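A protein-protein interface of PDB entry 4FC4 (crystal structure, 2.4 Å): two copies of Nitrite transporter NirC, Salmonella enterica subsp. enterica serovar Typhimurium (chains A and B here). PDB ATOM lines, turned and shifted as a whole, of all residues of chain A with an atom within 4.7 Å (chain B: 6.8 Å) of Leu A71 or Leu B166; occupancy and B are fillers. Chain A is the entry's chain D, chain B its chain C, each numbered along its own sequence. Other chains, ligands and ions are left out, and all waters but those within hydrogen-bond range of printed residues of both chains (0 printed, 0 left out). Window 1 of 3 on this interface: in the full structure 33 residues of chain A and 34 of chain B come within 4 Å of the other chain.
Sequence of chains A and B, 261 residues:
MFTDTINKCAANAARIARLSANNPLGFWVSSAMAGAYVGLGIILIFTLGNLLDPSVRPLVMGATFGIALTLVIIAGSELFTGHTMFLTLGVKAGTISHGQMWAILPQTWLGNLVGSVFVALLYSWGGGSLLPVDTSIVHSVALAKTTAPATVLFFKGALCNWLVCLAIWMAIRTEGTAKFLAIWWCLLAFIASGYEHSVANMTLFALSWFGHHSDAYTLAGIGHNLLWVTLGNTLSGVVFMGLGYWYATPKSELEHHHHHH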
ATOM      1  N   TYR A  37     -13.486   9.929 -21.255  1.00  0.00           N
ATOM      2  CA  TYR A  37     -13.964   9.995 -22.632  1.00  0.00           C
ATOM      3  C   TYR A  37     -14.839  11.225 -22.894  1.00  0.00           C
ATOM      4  O   TYR A  37     -14.608  11.915 -23.884  1.00  0.00           O
ATOM      5  CB  TYR A  37     -14.721   8.728 -22.987  1.00  0.00           C
ATOM      6  CG  TYR A  37     -13.910   7.470 -22.966  1.00  0.00           C
ATOM      7  CD1 TYR A  37     -12.505   7.491 -22.958  1.00  0.00           C
ATOM      8  CD2 TYR A  37     -14.559   6.238 -23.005  1.00  0.00           C
ATOM      9  CE1 TYR A  37     -11.775   6.314 -22.973  1.00  0.00           C
ATOM     10  CE2 TYR A  37     -13.848   5.058 -22.998  1.00  0.00           C
ATOM     11  CZ  TYR A  37     -12.460   5.088 -22.990  1.00  0.00           C
ATOM     12  OH  TYR A  37     -11.807   3.859 -23.009  1.00  0.00           O
ATOM     13  N   LEU A  40     -12.449  14.198 -22.807  1.00  0.00           N
ATOM     14  CA  LEU A  40     -11.653  14.428 -24.023  1.00  0.00           C
ATOM     15  C   LEU A  40     -12.457  15.236 -25.067  1.00  0.00           C
ATOM     16  O   LEU A  40     -11.898  16.093 -25.819  1.00  0.00           O
ATOM     17  CB  LEU A  40     -11.186  13.104 -24.583  1.00  0.00           C
ATOM     18  CG  LEU A  40     -10.091  12.441 -23.758  1.00  0.00           C
ATOM     19  CD1 LEU A  40     -10.191  10.956 -24.002  1.00  0.00           C
ATOM     20  CD2 LEU A  40      -8.697  12.939 -24.147  1.00  0.00           C
ATOM     21  N   ILE A  67     -17.950  12.951 -30.538  1.00  0.00           N
ATOM     22  CA  ILE A  67     -16.931  12.021 -30.075  1.00  0.00           C
ATOM     23  C   ILE A  67     -17.205  11.561 -28.614  1.00  0.00           C
ATOM     24  O   ILE A  67     -16.938  10.413 -28.252  1.00  0.00           O
ATOM     25  CB  ILE A  67     -15.474  12.572 -30.186  1.00  0.00           C
ATOM     26  CG1 ILE A  67     -14.469  11.487 -29.756  1.00  0.00           C
ATOM     27  CG2 ILE A  67     -15.204  13.886 -29.397  1.00  0.00           C
ATOM     28  CD1 ILE A  67     -13.067  11.761 -30.249  1.00  0.00           C
ATOM     29  N   ALA A  68     -17.712  12.462 -27.792  1.00  0.00           N
ATOM     30  CA  ALA A  68     -17.832  12.205 -26.346  1.00  0.00           C
ATOM     31  C   ALA A  68     -18.630  10.952 -26.083  1.00  0.00           C
ATOM     32  O   ALA A  68     -18.134  10.035 -25.440  1.00  0.00           O
ATOM     33  CB  ALA A  68     -18.445  13.407 -25.635  1.00  0.00           C
ATOM     34  N   LEU A  69     -19.832  10.869 -26.630  1.00  0.00           N
ATOM     35  CA  LEU A  69     -20.673   9.689 -26.380  1.00  0.00           C
ATOM     36  C   LEU A  69     -20.306   8.529 -27.300  1.00  0.00           C
ATOM     37  O   LEU A  69     -20.537   7.395 -26.981  1.00  0.00           O
ATOM     38  CB  LEU A  69     -22.164  10.021 -26.515  1.00  0.00           C
ATOM     39  CG  LEU A  69     -23.190   8.985 -26.053  1.00  0.00           C
ATOM     40  CD1 LEU A  69     -23.120   8.670 -24.549  1.00  0.00           C
ATOM     41  CD2 LEU A  69     -24.610   9.457 -26.417  1.00  0.00           C
ATOM     42  N   THR A  70     -19.758   8.823 -28.453  1.00  0.00           N
ATOM     43  CA  THR A  70     -19.252   7.779 -29.337  1.00  0.00           C
ATOM     44  C   THR A  70     -18.223   6.880 -28.663  1.00  0.00           C
ATOM     45  O   THR A  70     -18.335   5.660 -28.711  1.00  0.00           O
ATOM     46  CB  THR A  70     -18.750   8.473 -30.591  1.00  0.00           C
ATOM     47  OG1 THR A  70     -19.852   9.238 -31.059  1.00  0.00           O
ATOM     48  CG2 THR A  70     -18.171   7.516 -31.725  1.00  0.00           C
ATOM     49  N   LEU A  71     -17.227   7.485 -28.037  1.00  0.00           N
ATOM     50  CA  LEU A  71     -16.254   6.790 -27.232  1.00  0.00           C
ATOM     51  C   LEU A  71     -16.980   5.956 -26.155  1.00  0.00           C
ATOM     52  O   LEU A  71     -16.717   4.747 -26.019  1.00  0.00           O
ATOM     53  CB  LEU A  71     -15.303   7.818 -26.584  1.00  0.00           C
ATOM     54  CG  LEU A  71     -14.258   8.580 -27.439  1.00  0.00           C
ATOM     55  CD1 LEU A  71     -13.445   9.597 -26.637  1.00  0.00           C
ATOM     56  CD2 LEU A  71     -13.328   7.640 -28.159  1.00  0.00           C
ATOM     57  N   VAL A  72     -17.897   6.605 -25.418  1.00  0.00           N
ATOM     58  CA  VAL A  72     -18.582   5.989 -24.297  1.00  0.00           C
ATOM     59  C   VAL A  72     -19.315   4.737 -24.732  1.00  0.00           C
ATOM     60  O   VAL A  72     -19.108   3.699 -24.156  1.00  0.00           O
ATOM     61  CB  VAL A  72     -19.595   6.962 -23.616  1.00  0.00           C
ATOM     62  CG1 VAL A  72     -20.554   6.182 -22.717  1.00  0.00           C
ATOM     63  CG2 VAL A  72     -18.868   8.110 -22.883  1.00  0.00           C
ATOM     64  N   ILE A  73     -20.138   4.850 -25.775  1.00  0.00           N
ATOM     65  CA  ILE A  73     -20.932   3.772 -26.287  1.00  0.00           C
ATOM     66  C   ILE A  73     -20.128   2.759 -27.150  1.00  0.00           C
ATOM     67  O   ILE A  73     -20.273   1.560 -26.972  1.00  0.00           O
ATOM     68  CB  ILE A  73     -22.183   4.306 -27.015  1.00  0.00           C
ATOM     69  CG1 ILE A  73     -23.169   4.941 -26.033  1.00  0.00           C
ATOM     70  CG2 ILE A  73     -22.889   3.230 -27.891  1.00  0.00           C
ATOM     71  CD1 ILE A  73     -24.321   5.634 -26.776  1.00  0.00           C
ATOM     72  N   ILE A  74     -19.305   3.210 -28.092  1.00  0.00           N
ATOM     73  CA  ILE A  74     -18.616   2.292 -29.007  1.00  0.00           C
ATOM     74  C   ILE A  74     -17.349   1.670 -28.379  1.00  0.00           C
ATOM     75  O   ILE A  74     -17.047   0.476 -28.543  1.00  0.00           O
ATOM     76  CB  ILE A  74     -18.349   3.023 -30.377  1.00  0.00           C
ATOM     77  CG1 ILE A  74     -19.664   3.621 -30.962  1.00  0.00           C
ATOM     78  CG2 ILE A  74     -17.655   2.102 -31.431  1.00  0.00           C
ATOM     79  CD1 ILE A  74     -20.701   2.550 -31.398  1.00  0.00           C
ATOM     80  N   ALA A  75     -16.590   2.471 -27.646  1.00  0.00           N
ATOM     81  CA  ALA A  75     -15.343   2.010 -27.018  1.00  0.00           C
ATOM     82  C   ALA A  75     -15.672   1.136 -25.830  1.00  0.00           C
ATOM     83  O   ALA A  75     -14.981   0.157 -25.604  1.00  0.00           O
ATOM     84  CB  ALA A  75     -14.472   3.187 -26.583  1.00  0.00           C
ATOM     85  N   GLY A  76     -16.737   1.501 -25.096  1.00  0.00           N
ATOM     86  CA  GLY A  76     -17.230   0.768 -23.964  1.00  0.00           C
ATOM     87  C   GLY A  76     -16.788   1.451 -22.685  1.00  0.00           C
ATOM     88  O   GLY A  76     -15.576   1.729 -22.530  1.00  0.00           O
ATOM     89  N   LEU B  69      -4.717   7.654 -39.989  1.00  0.00           N
ATOM     90  CA  LEU B  69      -4.946   6.360 -39.358  1.00  0.00           C
ATOM     91  C   LEU B  69      -5.851   5.537 -40.249  1.00  0.00           C
ATOM     92  O   LEU B  69      -5.886   4.300 -40.134  1.00  0.00           O
ATOM     93  CB  LEU B  69      -5.557   6.503 -37.982  1.00  0.00           C
ATOM     94  CG  LEU B  69      -5.604   5.262 -37.074  1.00  0.00           C
ATOM     95  CD1 LEU B  69      -4.250   4.606 -36.774  1.00  0.00           C
ATOM     96  CD2 LEU B  69      -6.307   5.664 -35.791  1.00  0.00           C
ATOM     97  N   MET B  85      -0.454  -0.755 -27.587  1.00  0.00           N
ATOM     98  CA  MET B  85      -1.688  -1.402 -27.144  1.00  0.00           C
ATOM     99  C   MET B  85      -1.766  -2.917 -27.461  1.00  0.00           C
ATOM    100  O   MET B  85      -2.056  -3.716 -26.581  1.00  0.00           O
ATOM    101  CB  MET B  85      -2.910  -0.668 -27.720  1.00  0.00           C
ATOM    102  CG  MET B  85      -4.231  -0.987 -27.009  1.00  0.00           C
ATOM    103  SD  MET B  85      -5.744  -0.349 -27.780  1.00  0.00           S
ATOM    104  CE  MET B  85      -5.439  -0.742 -29.511  1.00  0.00           C
ATOM    105  N   CYS B 160      -2.560  12.147 -26.695  1.00  0.00           N
ATOM    106  CA  CYS B 160      -2.658  11.766 -28.133  1.00  0.00           C
ATOM    107  C   CYS B 160      -2.932  10.260 -28.353  1.00  0.00           C
ATOM    108  O   CYS B 160      -3.957   9.870 -28.992  1.00  0.00           O
ATOM    109  CB  CYS B 160      -1.425  12.160 -28.917  1.00  0.00           C
ATOM    110  SG  CYS B 160      -1.282  11.268 -30.485  1.00  0.00           S
ATOM    111  N   ASN B 161      -2.041   9.426 -27.820  1.00  0.00           N
ATOM    112  CA  ASN B 161      -2.200   7.988 -28.014  1.00  0.00           C
ATOM    113  C   ASN B 161      -3.394   7.311 -27.314  1.00  0.00           C
ATOM    114  O   ASN B 161      -3.764   6.235 -27.682  1.00  0.00           O
ATOM    115  CB  ASN B 161      -0.905   7.223 -27.748  1.00  0.00           C
ATOM    116  CG  ASN B 161      -0.749   6.060 -28.701  1.00  0.00           C
ATOM    117  OD1 ASN B 161      -1.308   6.093 -29.802  1.00  0.00           O
ATOM    118  ND2 ASN B 161      -0.021   5.025 -28.289  1.00  0.00           N
ATOM    119  N   TRP B 162      -3.966   7.929 -26.286  1.00  0.00           N
ATOM    120  CA  TRP B 162      -5.258   7.467 -25.739  1.00  0.00           C
ATOM    121  C   TRP B 162      -6.268   7.477 -26.857  1.00  0.00           C
ATOM    122  O   TRP B 162      -6.800   6.422 -27.270  1.00  0.00           O
ATOM    123  CB  TRP B 162      -5.733   8.414 -24.609  1.00  0.00           C
ATOM    124  CG  TRP B 162      -6.600   7.759 -23.563  1.00  0.00           C
ATOM    125  CD1 TRP B 162      -7.246   6.524 -23.634  1.00  0.00           C
ATOM    126  CD2 TRP B 162      -7.000   8.320 -22.244  1.00  0.00           C
ATOM    127  NE1 TRP B 162      -7.968   6.287 -22.476  1.00  0.00           N
ATOM    128  CE2 TRP B 162      -7.870   7.309 -21.616  1.00  0.00           C
ATOM    129  CE3 TRP B 162      -6.732   9.512 -21.556  1.00  0.00           C
ATOM    130  CZ2 TRP B 162      -8.426   7.492 -20.339  1.00  0.00           C
ATOM    131  CZ3 TRP B 162      -7.279   9.675 -20.258  1.00  0.00           C
ATOM    132  CH2 TRP B 162      -8.107   8.685 -19.665  1.00  0.00           C
ATOM    133  N   LEU B 163      -6.527   8.689 -27.357  1.00  0.00           N
ATOM    134  CA  LEU B 163      -7.338   8.888 -28.558  1.00  0.00           C
ATOM    135  C   LEU B 163      -6.990   8.043 -29.809  1.00  0.00           C
ATOM    136  O   LEU B 163      -7.880   7.432 -30.398  1.00  0.00           O
ATOM    137  CB  LEU B 163      -7.429  10.365 -28.913  1.00  0.00           C
ATOM    138  CG  LEU B 163      -8.378  11.175 -28.082  1.00  0.00           C
ATOM    139  CD1 LEU B 163      -7.923  12.624 -28.181  1.00  0.00           C
ATOM    140  CD2 LEU B 163      -9.793  10.940 -28.598  1.00  0.00           C
ATOM    141  N   VAL B 164      -5.727   7.973 -30.198  1.00  0.00           N
ATOM    142  CA  VAL B 164      -5.408   7.183 -31.399  1.00  0.00           C
ATOM    143  C   VAL B 164      -5.636   5.696 -31.142  1.00  0.00           C
ATOM    144  O   VAL B 164      -6.129   4.992 -32.052  1.00  0.00           O
ATOM    145  CB  VAL B 164      -3.974   7.441 -31.958  1.00  0.00           C
ATOM    146  CG1 VAL B 164      -3.729   6.616 -33.229  1.00  0.00           C
ATOM    147  CG2 VAL B 164      -3.780   8.936 -32.242  1.00  0.00           C
ATOM    148  N   CYS B 165      -5.304   5.220 -29.932  1.00  0.00           N
ATOM    149  CA  CYS B 165      -5.645   3.844 -29.575  1.00  0.00           C
ATOM    150  C   CYS B 165      -7.166   3.624 -29.478  1.00  0.00           C
ATOM    151  O   CYS B 165      -7.678   2.535 -29.857  1.00  0.00           O
ATOM    152  CB  CYS B 165      -4.899   3.359 -28.305  1.00  0.00           C
ATOM    153  SG  CYS B 165      -3.172   2.964 -28.629  1.00  0.00           S
ATOM    154  N   LEU B 166      -7.886   4.633 -28.964  1.00  0.00           N
ATOM    155  CA  LEU B 166      -9.344   4.541 -28.918  1.00  0.00           C
ATOM    156  C   LEU B 166      -9.896   4.333 -30.360  1.00  0.00           C
ATOM    157  O   LEU B 166     -10.863   3.596 -30.555  1.00  0.00           O
ATOM    158  CB  LEU B 166      -9.952   5.756 -28.241  1.00  0.00           C
ATOM    159  CG  LEU B 166      -9.896   5.774 -26.711  1.00  0.00           C
ATOM    160  CD1 LEU B 166     -10.145   7.188 -26.197  1.00  0.00           C
ATOM    161  CD2 LEU B 166     -10.910   4.815 -26.117  1.00  0.00           C
ATOM    162  N   ALA B 167      -9.261   4.952 -31.350  1.00  0.00           N
ATOM    163  CA  ALA B 167      -9.686   4.796 -32.764  1.00  0.00           C
ATOM    164  C   ALA B 167      -9.447   3.361 -33.184  1.00  0.00           C
ATOM    165  O   ALA B 167     -10.307   2.750 -33.797  1.00  0.00           O
ATOM    166  CB  ALA B 167      -8.909   5.743 -33.727  1.00  0.00           C
ATOM    167  N   ILE B 168      -8.241   2.862 -32.881  1.00  0.00           N
ATOM    168  CA  ILE B 168      -7.848   1.515 -33.174  1.00  0.00           C
ATOM    169  C   ILE B 168      -8.838   0.521 -32.558  1.00  0.00           C
ATOM    170  O   ILE B 168      -9.374  -0.378 -33.284  1.00  0.00           O
ATOM    171  CB  ILE B 168      -6.376   1.227 -32.752  1.00  0.00           C
ATOM    172  CG1 ILE B 168      -5.436   2.105 -33.595  1.00  0.00           C
ATOM    173  CG2 ILE B 168      -6.018  -0.240 -33.009  1.00  0.00           C
ATOM    174  CD1 ILE B 168      -3.953   1.944 -33.326  1.00  0.00           C
ATOM    175  N   TRP B 169      -9.074   0.693 -31.251  1.00  0.00           N
ATOM    176  CA  TRP B 169     -10.021  -0.116 -30.479  1.00  0.00           C
ATOM    177  C   TRP B 169     -11.411  -0.080 -31.100  1.00  0.00           C
ATOM    178  O   TRP B 169     -12.026  -1.143 -31.384  1.00  0.00           O
ATOM    179  CB  TRP B 169      -9.992   0.383 -29.006  1.00  0.00           C
ATOM    180  CG  TRP B 169     -10.911  -0.278 -28.006  1.00  0.00           C
ATOM    181  CD1 TRP B 169     -12.156   0.174 -27.564  1.00  0.00           C
ATOM    182  CD2 TRP B 169     -10.663  -1.524 -27.224  1.00  0.00           C
ATOM    183  NE1 TRP B 169     -12.700  -0.695 -26.642  1.00  0.00           N
ATOM    184  CE2 TRP B 169     -11.844  -1.722 -26.380  1.00  0.00           C
ATOM    185  CE3 TRP B 169      -9.611  -2.448 -27.143  1.00  0.00           C
ATOM    186  CZ2 TRP B 169     -11.966  -2.817 -25.529  1.00  0.00           C
ATOM    187  CZ3 TRP B 169      -9.747  -3.554 -26.271  1.00  0.00           C
ATOM    188  CH2 TRP B 169     -10.895  -3.731 -25.490  1.00  0.00           C
ATOM    189  N   MET B 170     -11.930   1.132 -31.340  1.00  0.00           N
ATOM    190  CA  MET B 170     -13.287   1.299 -31.895  1.00  0.00           C
ATOM    191  C   MET B 170     -13.420   0.736 -33.316  1.00  0.00           C
ATOM    192  O   MET B 170     -14.434   0.128 -33.649  1.00  0.00           O
ATOM    193  CB  MET B 170     -13.725   2.764 -31.844  1.00  0.00           C
ATOM    194  CG  MET B 170     -14.173   3.282 -30.479  1.00  0.00           C
ATOM    195  SD  MET B 170     -14.948   4.923 -30.496  1.00  0.00           S
ATOM    196  CE  MET B 170     -13.618   5.950 -31.086  1.00  0.00           C
ATOM    197  N   ALA B 171     -12.401   0.914 -34.165  1.00  0.00           N
ATOM    198  CA  ALA B 171     -12.427   0.324 -35.519  1.00  0.00           C
ATOM    199  C   ALA B 171     -12.554  -1.236 -35.441  1.00  0.00           C
ATOM    200  O   ALA B 171     -13.275  -1.866 -36.216  1.00  0.00           O
ATOM    201  CB  ALA B 171     -11.194   0.768 -36.311  1.00  0.00           C
ATOM    202  N   ILE B 172     -11.923  -1.844 -34.428  1.00  0.00           N
ATOM    203  CA  ILE B 172     -11.966  -3.307 -34.276  1.00  0.00           C
ATOM    204  C   ILE B 172     -13.332  -3.694 -33.811  1.00  0.00           C
ATOM    205  O   ILE B 172     -13.826  -4.708 -34.230  1.00  0.00           O
ATOM    206  CB  ILE B 172     -10.899  -3.871 -33.297  1.00  0.00           C
ATOM    207  CG1 ILE B 172      -9.536  -3.890 -33.994  1.00  0.00           C
ATOM    208  CG2 ILE B 172     -11.296  -5.266 -32.752  1.00  0.00           C
ATOM    209  CD1 ILE B 172      -8.368  -3.587 -33.076  1.00  0.00           C
ATOM    210  N   ALA B 182     -14.955   6.440 -36.580  1.00  0.00           N
ATOM    211  CA  ALA B 182     -14.322   6.382 -35.303  1.00  0.00           C
ATOM    212  C   ALA B 182     -12.944   6.987 -35.465  1.00  0.00           C
ATOM    213  O   ALA B 182     -12.464   7.730 -34.577  1.00  0.00           O
ATOM    214  CB  ALA B 182     -14.221   4.940 -34.808  1.00  0.00           C
ATOM    215  N   TRP B 185     -13.075  10.875 -35.840  1.00  0.00           N
ATOM    216  CA  TRP B 185     -13.390  11.553 -34.588  1.00  0.00           C
ATOM    217  C   TRP B 185     -12.147  11.787 -33.781  1.00  0.00           C
ATOM    218  O   TRP B 185     -11.835  12.904 -33.321  1.00  0.00           O
ATOM    219  CB  TRP B 185     -14.362  10.685 -33.756  1.00  0.00           C
ATOM    220  CG  TRP B 185     -15.788  11.066 -33.996  1.00  0.00           C
ATOM    221  CD1 TRP B 185     -16.826  10.247 -34.393  1.00  0.00           C
ATOM    222  CD2 TRP B 185     -16.378  12.413 -33.894  1.00  0.00           C
ATOM    223  NE1 TRP B 185     -17.968  10.969 -34.548  1.00  0.00           N
ATOM    224  CE2 TRP B 185     -17.772  12.268 -34.284  1.00  0.00           C
ATOM    225  CE3 TRP B 185     -15.883  13.688 -33.563  1.00  0.00           C
ATOM    226  CZ2 TRP B 185     -18.641  13.338 -34.306  1.00  0.00           C
ATOM    227  CZ3 TRP B 185     -16.752  14.764 -33.592  1.00  0.00           C
ATOM    228  CH2 TRP B 185     -18.103  14.596 -33.944  1.00  0.00           C
ATOM    229  N   CYS B 186     -11.407  10.707 -33.618  1.00  0.00           N
ATOM    230  CA  CYS B 186     -10.293  10.647 -32.679  1.00  0.00           C
ATOM    231  C   CYS B 186      -9.101  11.474 -33.194  1.00  0.00           C
ATOM    232  O   CYS B 186      -8.425  12.140 -32.402  1.00  0.00           O
ATOM    233  CB  CYS B 186      -9.870   9.170 -32.522  1.00  0.00           C
ATOM    234  SG  CYS B 186     -11.026   8.267 -31.489  1.00  0.00           S
ATOM    235  N   ALA B 189     -10.010  15.001 -32.663  1.00  0.00           N
ATOM    236  CA  ALA B 189      -9.909  15.398 -31.249  1.00  0.00           C
ATOM    237  C   ALA B 189      -8.449  15.603 -30.880  1.00  0.00           C
ATOM    238  O   ALA B 189      -8.093  16.595 -30.176  1.00  0.00           O
ATOM    239  CB  ALA B 189     -10.572  14.373 -30.326  1.00  0.00           C
ATOM    240  N   MET B 241      -5.109   2.134 -22.168  1.00  0.00           N
ATOM    241  CA  MET B 241      -5.790   1.233 -23.125  1.00  0.00           C
ATOM    242  C   MET B 241      -5.554  -0.267 -22.922  1.00  0.00           C
ATOM    243  O   MET B 241      -6.521  -1.009 -22.686  1.00  0.00           O
ATOM    244  CB  MET B 241      -5.547   1.650 -24.586  1.00  0.00           C
ATOM    245  CG  MET B 241      -6.260   2.935 -24.981  1.00  0.00           C
ATOM    246  SD  MET B 241      -8.050   2.743 -25.025  1.00  0.00           S
ATOM    247  CE  MET B 241      -8.464   3.325 -23.369  1.00  0.00           C
ATOM    248  N   TYR B 245      -8.430  -1.666 -20.377  1.00  0.00           N
ATOM    249  CA  TYR B 245      -9.476  -2.631 -20.786  1.00  0.00           C
ATOM    250  C   TYR B 245      -9.334  -4.050 -20.213  1.00  0.00           C
ATOM    251  O   TYR B 245     -10.354  -4.708 -19.907  1.00  0.00           O
ATOM    252  CB  TYR B 245      -9.766  -2.630 -22.295  1.00  0.00           C
ATOM    253  CG  TYR B 245     -10.688  -1.489 -22.686  1.00  0.00           C
ATOM    254  CD1 TYR B 245     -12.047  -1.522 -22.372  1.00  0.00           C
ATOM    255  CD2 TYR B 245     -10.181  -0.339 -23.309  1.00  0.00           C
ATOM    256  CE1 TYR B 245     -12.883  -0.451 -22.692  1.00  0.00           C
ATOM    257  CE2 TYR B 245     -11.002   0.729 -23.638  1.00  0.00           C
ATOM    258  CZ  TYR B 245     -12.351   0.669 -23.330  1.00  0.00           C
ATOM    259  OH  TYR B 245     -13.162   1.715 -23.699  1.00  0.00           O
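NE1 of Trp B169 lies within hydrogen-bond range of O of Ala A75, 2.6 Å away. OH of Tyr B245 sits at hydrogen-bond distance from OH of Tyr A37, 2.6 Å away. The side-chain hydroxyl (OH) of Tyr B245 is in hydrogen-bond range of the backbone carbonyl oxygen (O) of Ala A75, at 3.1 Å. O of Gly A76 is in hydrogen-bond range of OH of Tyr B245, 2.7 Å away.
The backbone carbonyl oxygen of Leu B163 sits close to the side-chain sulfur of Cys B186 (3.4 Å). The backbone NH (N) of Ala B167 is in hydrogen-bond range of the side-chain sulfur (SG) of Cys B186, at 3.8 Å. The side-chain sulfur of Cys B186 is in hydrogen-bond range of the backbone carbonyl oxygen of Ala B182 (3.4 Å). O of Leu A71 sits at hydrogen-bond distance from N of Gly A76, at 3.4 Å.
Among the printed residues, merely in contact across the chains: Tyr A37 with Leu B166 (3.4 Å), Leu A71 with Met B170 (3.4 Å), Tyr A37 with Met B241 (3.4 Å), Ile A67 with Trp B185 (3.5 Å), Ile A67 with Ala B189 (3.6 Å), Ile A67 with Leu B163 (3.8 Å), Leu A71 with Leu B166 (3.8 Å), Ile A74 with Met B170 (3.8 Å), Ala A75 with Met B170 (3.8 Å), Tyr A37 with Trp B162 (3.8 Å), Ile A67 with Cys B186 (3.9 Å), Thr A70 with Met B170 (3.9 Å) and Ala A75 with Leu B166 (3.9 Å).
Leu A40 touches none of the printed residues of chain B. Ala A68 touches none of the printed residues of chain B. Printed residues of chain B within 4 Å of Gly A76: Tyr B245. Of the printed residues of chain A, Trp B162 touches Tyr A37. Leu B166 touches just these residues of chain A: Tyr A37, Leu A71 and Ala A75. Printed residues of chain A within 4 Å of Ala B189: Ile A67. Of the printed residues of chain A, Met B241 touches Tyr A37. The nearest residue of chain A that does not touch Leu B166 is Leu A40 (4.4 Å). The nearest printed residue of chain B that does not touch Tyr A37 is Trp B169 (5.9 Å).
Hydrophobic or aromatic side chains of chain A within 4 Å of the printed part of chain B: Tyr A37, Ile A67, Leu A71, Ile A74 and Ala A75. Of the 21 printed residues of chain B, 10 touch a printed residue of chain A. Hydrophobic or aromatic side chains of chain B that line the printed part of chain A: Trp B162, Leu B163, Leu B166, Trp B169, Met B170, Trp B185, Ala B189, Met B241 and Tyr B245. Among the printed residues, no Asp or Glu carboxylate lies within 4 Å of a Lys or Arg side-chain nitrogen of the other chain.
Position printed for both chains: 69.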
